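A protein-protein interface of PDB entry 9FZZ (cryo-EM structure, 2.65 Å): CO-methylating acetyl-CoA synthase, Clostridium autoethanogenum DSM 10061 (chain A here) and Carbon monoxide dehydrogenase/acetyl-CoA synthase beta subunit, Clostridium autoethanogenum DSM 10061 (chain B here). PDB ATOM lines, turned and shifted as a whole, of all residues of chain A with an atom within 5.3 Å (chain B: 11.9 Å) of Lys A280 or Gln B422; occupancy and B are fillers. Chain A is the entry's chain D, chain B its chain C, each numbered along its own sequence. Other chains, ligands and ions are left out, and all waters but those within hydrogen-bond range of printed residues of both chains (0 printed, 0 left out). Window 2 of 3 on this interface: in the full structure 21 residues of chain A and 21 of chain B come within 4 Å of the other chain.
Lys A280 touches just one residue of chain B: Gln B422 (3.8 Å). No residue of chain B comes within 4 Å of Ser A282. No residue of chain B comes within 4 Å of Leu A283. Glu A284 touches four residues of chain B. Printed residues of chain A within 4 Å of Val B419: Glu A284. Of the printed residues of chain A, Thr B421 touches Glu A284. Gln B422 touches five residues of chain A. Of the printed residues of chain A, Ile B423 touches Gln A272 (3.4 Å) and Thr A281 (3.6 Å). The nearest residue of chain B that does not touch Lys A280 is Asn B420 (5.3 Å). The nearest printed residue of chain A that does not touch Val B419 is Ala A285 (8.3 Å).
The backbone carbonyl oxygen (O) of Gln B422 is in hydrogen-bond range of the side-chain amide nitrogen (NE2) of Gln A272 (3.1 Å). O of Gln B422 sits at hydrogen-bond distance from NZ of Lys A277 (2.9 Å). ND2 of Asn B420 lies within hydrogen-bond range of O of Thr A281, 3.2 Å away. The side-chain carboxylate (OE1) of Glu A284 sits close to the side-chain amide oxygen (OD1) of Asn B420 (3.3 Å). OE2 of Glu A284 is in hydrogen-bond range of N of Thr B421 (2.6 Å). The side-chain carboxylate of Glu A284 sits at hydrogen-bond distance from the backbone NH of Gln B422 (3.4 Å).
OD2 of Asp A154 is in salt-bridge range of NZ of Lys A280 (3.6 Å). The side-chain hydroxyl (OG1) of Thr A281 sits at hydrogen-bond distance from the side-chain amide nitrogen (NE2) of Gln A272, 3.1 Å away. The side-chain amino group (NZ) of Lys A280 is in hydrogen-bond range of the backbone carbonyl oxygen (O) of Asp A276 (2.8 Å). The backbone carbonyl oxygen (O) of Lys A277 sits at hydrogen-bond distance from the side-chain hydroxyl (OG1) of Thr A281 (2.5 Å). The side-chain amide oxygen of Asn B420 lies within hydrogen-bond range of the backbone NH of Gln B422, at 3.0 Å.
Of the 12 printed residues of chain B, 5 touch a printed residue of chain A. Of the 14 printed residues of chain A, 6 touch a printed residue of chain B. Printed residues of chain A that touch a printed residue of chain B: Gln A272, Lys A277, Lys A280, Thr A281, Glu A284 and Ala A285. Hydrophobic or aromatic side chains of chain A within 4 Å of the printed part of chain B: Ala A285. Among the printed residues, 12 pairs touch across the chains. Among the printed residues, no Asp or Glu carboxylate lies within 4 Å of a Lys or Arg side-chain nitrogen of the other chain.
Among the printed residues, pairs that only touch across the chains: Gln A272 with Ile B423, Lys A280 with Gln B422, Thr A281 with Gln B422, Thr A281 with Ile B423, Glu A284 with Val B419 and Ala A285 with Asn B420.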
ATOM      1  N   LYS A 150      11.203  16.630 -15.821  1.00  0.00           N
ATOM      2  CA  LYS A 150      10.675  17.380 -14.687  1.00  0.00           C
ATOM      3  C   LYS A 150      11.801  17.887 -13.794  1.00  0.00           C
ATOM      4  O   LYS A 150      11.820  19.061 -13.408  1.00  0.00           O
ATOM      5  CB  LYS A 150       9.698  16.496 -13.902  1.00  0.00           C
ATOM      6  CG  LYS A 150       9.069  17.179 -12.675  1.00  0.00           C
ATOM      7  CD  LYS A 150       9.898  16.935 -11.394  1.00  0.00           C
ATOM      8  CE  LYS A 150       9.609  18.014 -10.334  1.00  0.00           C
ATOM      9  NZ  LYS A 150      10.629  18.010  -9.229  1.00  0.00           N
ATOM     10  N   ASP A 154      12.936  21.702 -13.491  1.00  0.00           N
ATOM     11  CA  ASP A 154      12.855  22.287 -12.159  1.00  0.00           C
ATOM     12  C   ASP A 154      14.139  23.031 -11.806  1.00  0.00           C
ATOM     13  O   ASP A 154      14.091  24.160 -11.306  1.00  0.00           O
ATOM     14  CB  ASP A 154      12.561  21.181 -11.147  1.00  0.00           C
ATOM     15  CG  ASP A 154      12.219  21.715  -9.771  1.00  0.00           C
ATOM     16  OD1 ASP A 154      12.210  22.950  -9.606  1.00  0.00           O
ATOM     17  OD2 ASP A 154      11.953  20.908  -8.860  1.00  0.00           O
ATOM     18  N   LYS A 158      14.762  27.380 -11.675  1.00  0.00           N
ATOM     19  CA  LYS A 158      15.353  27.998 -10.499  1.00  0.00           C
ATOM     20  C   LYS A 158      16.643  28.746 -10.803  1.00  0.00           C
ATOM     21  O   LYS A 158      17.278  29.263  -9.878  1.00  0.00           O
ATOM     22  CB  LYS A 158      15.620  26.936  -9.426  1.00  0.00           C
ATOM     23  CG  LYS A 158      14.344  26.341  -8.848  1.00  0.00           C
ATOM     24  CD  LYS A 158      14.661  25.476  -7.626  1.00  0.00           C
ATOM     25  CE  LYS A 158      13.428  24.693  -7.164  1.00  0.00           C
ATOM     26  NZ  LYS A 158      12.260  25.593  -6.895  1.00  0.00           N
ATOM     27  N   GLN A 272      18.224   9.402  -2.247  1.00  0.00           N
ATOM     28  CA  GLN A 272      16.892  10.000  -2.267  1.00  0.00           C
ATOM     29  C   GLN A 272      16.141   9.311  -3.402  1.00  0.00           C
ATOM     30  O   GLN A 272      16.384   9.601  -4.578  1.00  0.00           O
ATOM     31  CB  GLN A 272      16.962  11.516  -2.467  1.00  0.00           C
ATOM     32  CG  GLN A 272      15.586  12.187  -2.610  1.00  0.00           C
ATOM     33  CD  GLN A 272      14.703  11.939  -1.386  1.00  0.00           C
ATOM     34  OE1 GLN A 272      13.901  11.016  -1.375  1.00  0.00           O
ATOM     35  NE2 GLN A 272      14.869  12.756  -0.342  1.00  0.00           N
ATOM     36  N   ASP A 276      10.308  13.421  -6.625  1.00  0.00           N
ATOM     37  CA  ASP A 276       9.616  14.678  -6.376  1.00  0.00           C
ATOM     38  C   ASP A 276      10.320  15.550  -5.354  1.00  0.00           C
ATOM     39  O   ASP A 276       9.996  16.735  -5.249  1.00  0.00           O
ATOM     40  CB  ASP A 276       8.182  14.409  -5.917  1.00  0.00           C
ATOM     41  CG  ASP A 276       7.296  13.904  -7.035  1.00  0.00           C
ATOM     42  OD1 ASP A 276       7.568  14.266  -8.198  1.00  0.00           O
ATOM     43  OD2 ASP A 276       6.344  13.148  -6.764  1.00  0.00           O
ATOM     44  N   LYS A 277      11.289  15.005  -4.625  1.00  0.00           N
ATOM     45  CA  LYS A 277      12.030  15.761  -3.627  1.00  0.00           C
ATOM     46  C   LYS A 277      13.525  15.831  -3.906  1.00  0.00           C
ATOM     47  O   LYS A 277      14.264  16.383  -3.087  1.00  0.00           O
ATOM     48  CB  LYS A 277      11.803  15.162  -2.233  1.00  0.00           C
ATOM     49  CG  LYS A 277      10.355  15.259  -1.748  1.00  0.00           C
ATOM     50  CD  LYS A 277      10.261  14.962  -0.241  1.00  0.00           C
ATOM     51  CE  LYS A 277      10.880  13.595   0.093  1.00  0.00           C
ATOM     52  NZ  LYS A 277      10.807  13.295   1.560  1.00  0.00           N
ATOM     53  N   MET A 278      13.984  15.304  -5.043  1.00  0.00           N
ATOM     54  CA  MET A 278      15.416  15.282  -5.330  1.00  0.00           C
ATOM     55  C   MET A 278      15.983  16.690  -5.478  1.00  0.00           C
ATOM     56  O   MET A 278      17.081  16.973  -4.987  1.00  0.00           O
ATOM     57  CB  MET A 278      15.686  14.453  -6.592  1.00  0.00           C
ATOM     58  CG  MET A 278      17.164  14.461  -7.041  1.00  0.00           C
ATOM     59  SD  MET A 278      18.304  13.888  -5.759  1.00  0.00           S
ATOM     60  CE  MET A 278      18.160  12.109  -5.882  1.00  0.00           C
ATOM     61  N   VAL A 279      15.256  17.587  -6.147  1.00  0.00           N
ATOM     62  CA  VAL A 279      15.724  18.964  -6.297  1.00  0.00           C
ATOM     63  C   VAL A 279      15.853  19.640  -4.936  1.00  0.00           C
ATOM     64  O   VAL A 279      16.887  20.236  -4.616  1.00  0.00           O
ATOM     65  CB  VAL A 279      14.782  19.741  -7.234  1.00  0.00           C
ATOM     66  CG1 VAL A 279      15.068  21.247  -7.201  1.00  0.00           C
ATOM     67  CG2 VAL A 279      14.888  19.212  -8.672  1.00  0.00           C
ATOM     68  N   LYS A 280      14.837  19.500  -4.081  1.00  0.00           N
ATOM     69  CA  LYS A 280      14.902  20.121  -2.757  1.00  0.00           C
ATOM     70  C   LYS A 280      15.982  19.478  -1.896  1.00  0.00           C
ATOM     71  O   LYS A 280      16.657  20.166  -1.123  1.00  0.00           O
ATOM     72  CB  LYS A 280      13.551  20.038  -2.044  1.00  0.00           C
ATOM     73  CG  LYS A 280      12.515  21.071  -2.523  1.00  0.00           C
ATOM     74  CD  LYS A 280      12.142  20.879  -4.009  1.00  0.00           C
ATOM     75  CE  LYS A 280      11.486  19.504  -4.249  1.00  0.00           C
ATOM     76  NZ  LYS A 280      11.294  19.227  -5.704  1.00  0.00           N
ATOM     77  N   THR A 281      16.174  18.163  -2.026  1.00  0.00           N
ATOM     78  CA  THR A 281      17.241  17.502  -1.284  1.00  0.00           C
ATOM     79  C   THR A 281      18.601  18.033  -1.707  1.00  0.00           C
ATOM     80  O   THR A 281      19.481  18.243  -0.866  1.00  0.00           O
ATOM     81  CB  THR A 281      17.166  15.991  -1.519  1.00  0.00           C
ATOM     82  OG1 THR A 281      15.817  15.536  -1.336  1.00  0.00           O
ATOM     83  CG2 THR A 281      18.108  15.224  -0.583  1.00  0.00           C
ATOM     84  N   SER A 282      18.798  18.242  -3.012  1.00  0.00           N
ATOM     85  CA  SER A 282      20.100  18.700  -3.490  1.00  0.00           C
ATOM     86  C   SER A 282      20.375  20.133  -3.052  1.00  0.00           C
ATOM     87  O   SER A 282      21.495  20.463  -2.651  1.00  0.00           O
ATOM     88  CB  SER A 282      20.179  18.589  -5.018  1.00  0.00           C
ATOM     89  OG  SER A 282      19.959  17.253  -5.459  1.00  0.00           O
ATOM     90  N   LEU A 283      19.358  20.996  -3.109  1.00  0.00           N
ATOM     91  CA  LEU A 283      19.561  22.385  -2.709  1.00  0.00           C
ATOM     92  C   LEU A 283      19.936  22.469  -1.238  1.00  0.00           C
ATOM     93  O   LEU A 283      20.807  23.254  -0.854  1.00  0.00           O
ATOM     94  CB  LEU A 283      18.305  23.213  -3.002  1.00  0.00           C
ATOM     95  CG  LEU A 283      17.858  23.222  -4.475  1.00  0.00           C
ATOM     96  CD1 LEU A 283      16.602  24.074  -4.633  1.00  0.00           C
ATOM     97  CD2 LEU A 283      18.961  23.704  -5.425  1.00  0.00           C
ATOM     98  N   GLU A 284      19.278  21.670  -0.397  1.00  0.00           N
ATOM     99  CA  GLU A 284      19.661  21.625   1.009  1.00  0.00           C
ATOM    100  C   GLU A 284      21.058  21.048   1.190  1.00  0.00           C
ATOM    101  O   GLU A 284      21.844  21.559   1.994  1.00  0.00           O
ATOM    102  CB  GLU A 284      18.649  20.817   1.821  1.00  0.00           C
ATOM    103  CG  GLU A 284      19.062  20.703   3.292  1.00  0.00           C
ATOM    104  CD  GLU A 284      18.106  19.862   4.110  1.00  0.00           C
ATOM    105  OE1 GLU A 284      17.001  19.578   3.617  1.00  0.00           O
ATOM    106  OE2 GLU A 284      18.463  19.476   5.242  1.00  0.00           O
ATOM    107  N   ALA A 285      21.393  19.996   0.438  1.00  0.00           N
ATOM    108  CA  ALA A 285      22.694  19.350   0.596  1.00  0.00           C
ATOM    109  C   ALA A 285      23.830  20.256   0.158  1.00  0.00           C
ATOM    110  O   ALA A 285      24.927  20.184   0.716  1.00  0.00           O
ATOM    111  CB  ALA A 285      22.737  18.025  -0.176  1.00  0.00           C
ATOM    112  N   ASP B 416      21.748  14.939  14.557  1.00  0.00           N
ATOM    113  CA  ASP B 416      20.675  15.520  13.757  1.00  0.00           C
ATOM    114  C   ASP B 416      21.159  16.623  12.821  1.00  0.00           C
ATOM    115  O   ASP B 416      20.501  16.896  11.816  1.00  0.00           O
ATOM    116  CB  ASP B 416      19.574  16.083  14.660  1.00  0.00           C
ATOM    117  CG  ASP B 416      18.614  15.017  15.160  1.00  0.00           C
ATOM    118  OD1 ASP B 416      18.851  13.825  14.872  1.00  0.00           O
ATOM    119  OD2 ASP B 416      17.629  15.365  15.834  1.00  0.00           O
ATOM    120  N   LYS B 417      22.310  17.236  13.101  1.00  0.00           N
ATOM    121  CA  LYS B 417      22.785  18.315  12.239  1.00  0.00           C
ATOM    122  C   LYS B 417      23.147  17.808  10.850  1.00  0.00           C
ATOM    123  O   LYS B 417      22.935  18.515   9.860  1.00  0.00           O
ATOM    124  CB  LYS B 417      23.980  19.024  12.884  1.00  0.00           C
ATOM    125  CG  LYS B 417      24.677  19.979  11.914  1.00  0.00           C
ATOM    126  CD  LYS B 417      25.615  20.937  12.640  1.00  0.00           C
ATOM    127  CE  LYS B 417      26.772  20.171  13.271  1.00  0.00           C
ATOM    128  NZ  LYS B 417      28.000  21.016  13.252  1.00  0.00           N
ATOM    129  N   VAL B 418      23.711  16.602  10.745  1.00  0.00           N
ATOM    130  CA  VAL B 418      24.199  16.092   9.466  1.00  0.00           C
ATOM    131  C   VAL B 418      23.105  15.282   8.760  1.00  0.00           C
ATOM    132  O   VAL B 418      23.386  14.542   7.814  1.00  0.00           O
ATOM    133  CB  VAL B 418      25.482  15.253   9.634  1.00  0.00           C
ATOM    134  CG1 VAL B 418      26.633  16.117  10.183  1.00  0.00           C
ATOM    135  CG2 VAL B 418      25.241  14.023  10.526  1.00  0.00           C
ATOM    136  N   VAL B 419      21.851  15.430   9.193  1.00  0.00           N
ATOM    137  CA  VAL B 419      20.717  14.755   8.568  1.00  0.00           C
ATOM    138  C   VAL B 419      20.083  15.709   7.560  1.00  0.00           C
ATOM    139  O   VAL B 419      19.649  16.809   7.925  1.00  0.00           O
ATOM    140  CB  VAL B 419      19.683  14.296   9.613  1.00  0.00           C
ATOM    141  CG1 VAL B 419      18.447  13.705   8.921  1.00  0.00           C
ATOM    142  CG2 VAL B 419      20.290  13.269  10.582  1.00  0.00           C
ATOM    143  N   ASN B 420      19.993  15.279   6.304  1.00  0.00           N
ATOM    144  CA  ASN B 420      19.268  16.059   5.306  1.00  0.00           C
ATOM    145  C   ASN B 420      17.785  16.054   5.660  1.00  0.00           C
ATOM    146  O   ASN B 420      17.180  14.991   5.831  1.00  0.00           O
ATOM    147  CB  ASN B 420      19.501  15.496   3.899  1.00  0.00           C
ATOM    148  CG  ASN B 420      19.016  16.446   2.795  1.00  0.00           C
ATOM    149  OD1 ASN B 420      17.820  16.587   2.582  1.00  0.00           O
ATOM    150  ND2 ASN B 420      19.950  17.103   2.095  1.00  0.00           N
ATOM    151  N   THR B 421      17.190  17.249   5.742  1.00  0.00           N
ATOM    152  CA  THR B 421      15.798  17.368   6.170  1.00  0.00           C
ATOM    153  C   THR B 421      14.867  16.660   5.200  1.00  0.00           C
ATOM    154  O   THR B 421      13.878  16.050   5.614  1.00  0.00           O
ATOM    155  CB  THR B 421      15.400  18.840   6.309  1.00  0.00           C
ATOM    156  OG1 THR B 421      16.194  19.482   7.317  1.00  0.00           O
ATOM    157  CG2 THR B 421      13.940  18.971   6.699  1.00  0.00           C
ATOM    158  N   GLN B 422      15.155  16.744   3.902  1.00  0.00           N
ATOM    159  CA  GLN B 422      14.307  16.116   2.893  1.00  0.00           C
ATOM    160  C   GLN B 422      14.406  14.594   2.898  1.00  0.00           C
ATOM    161  O   GLN B 422      13.595  13.941   2.231  1.00  0.00           O
ATOM    162  CB  GLN B 422      14.665  16.645   1.496  1.00  0.00           C
ATOM    163  CG  GLN B 422      14.609  18.179   1.370  1.00  0.00           C
ATOM    164  CD  GLN B 422      13.223  18.739   1.684  1.00  0.00           C
ATOM    165  OE1 GLN B 422      12.226  18.279   1.145  1.00  0.00           O
ATOM    166  NE2 GLN B 422      13.160  19.731   2.578  1.00  0.00           N
ATOM    167  N   ILE B 423      15.378  14.012   3.599  1.00  0.00           N
ATOM    168  CA  ILE B 423      15.549  12.562   3.665  1.00  0.00           C
ATOM    169  C   ILE B 423      15.119  12.019   5.025  1.00  0.00           C
ATOM    170  O   ILE B 423      14.200  11.203   5.116  1.00  0.00           O
ATOM    171  CB  ILE B 423      17.004  12.154   3.329  1.00  0.00           C
ATOM    172  CG1 ILE B 423      17.390  12.649   1.927  1.00  0.00           C
ATOM    173  CG2 ILE B 423      17.167  10.629   3.445  1.00  0.00           C
ATOM    174  CD1 ILE B 423      18.876  12.478   1.614  1.00  0.00           C
ATOM    175  N   GLY B 424      15.781  12.454   6.092  1.00  0.00           N
ATOM    176  CA  GLY B 424      15.520  11.958   7.421  1.00  0.00           C
ATOM    177  C   GLY B 424      15.962  10.516   7.581  1.00  0.00           C
ATOM    178  O   GLY B 424      16.719   9.989   6.761  1.00  0.00           O
ATOM    179  N   PRO B 425      15.507   9.853   8.650  1.00  0.00           N
ATOM    180  CA  PRO B 425      14.662  10.373   9.743  1.00  0.00           C
ATOM    181  C   PRO B 425      15.487  11.166  10.746  1.00  0.00           C
ATOM    182  O   PRO B 425      16.713  11.159  10.695  1.00  0.00           O
ATOM    183  CB  PRO B 425      14.062   9.090  10.348  1.00  0.00           C
ATOM    184  CG  PRO B 425      15.186   8.072  10.183  1.00  0.00           C
ATOM    185  CD  PRO B 425      15.829   8.422   8.845  1.00  0.00           C
ATOM    186  N   MET B 426      14.826  11.891  11.641  1.00  0.00           N
ATOM    187  CA  MET B 426      15.495  12.630  12.694  1.00  0.00           C
ATOM    188  C   MET B 426      15.479  11.822  13.985  1.00  0.00           C
ATOM    189  O   MET B 426      14.725  10.854  14.135  1.00  0.00           O
ATOM    190  CB  MET B 426      14.815  13.994  12.914  1.00  0.00           C
ATOM    191  CG  MET B 426      14.943  14.968  11.717  1.00  0.00           C
ATOM    192  SD  MET B 426      16.643  15.508  11.449  1.00  0.00           S
ATOM    193  CE  MET B 426      16.473  16.595  10.043  1.00  0.00           C
ATOM    194  N   LYS B 430      21.112   6.913  13.122  1.00  0.00           N
ATOM    195  CA  LYS B 430      21.384   6.565  11.731  1.00  0.00           C
ATOM    196  C   LYS B 430      22.614   7.247  11.147  1.00  0.00           C
ATOM    197  O   LYS B 430      23.358   6.573  10.417  1.00  0.00           O
ATOM    198  CB  LYS B 430      20.157   6.860  10.867  1.00  0.00           C
ATOM    199  CG  LYS B 430      20.311   6.351   9.437  1.00  0.00           C
ATOM    200  CD  LYS B 430      19.019   6.551   8.657  1.00  0.00           C
ATOM    201  CE  LYS B 430      19.090   5.856   7.296  1.00  0.00           C
ATOM    202  NZ  LYS B 430      20.218   6.400   6.463  1.00  0.00           N
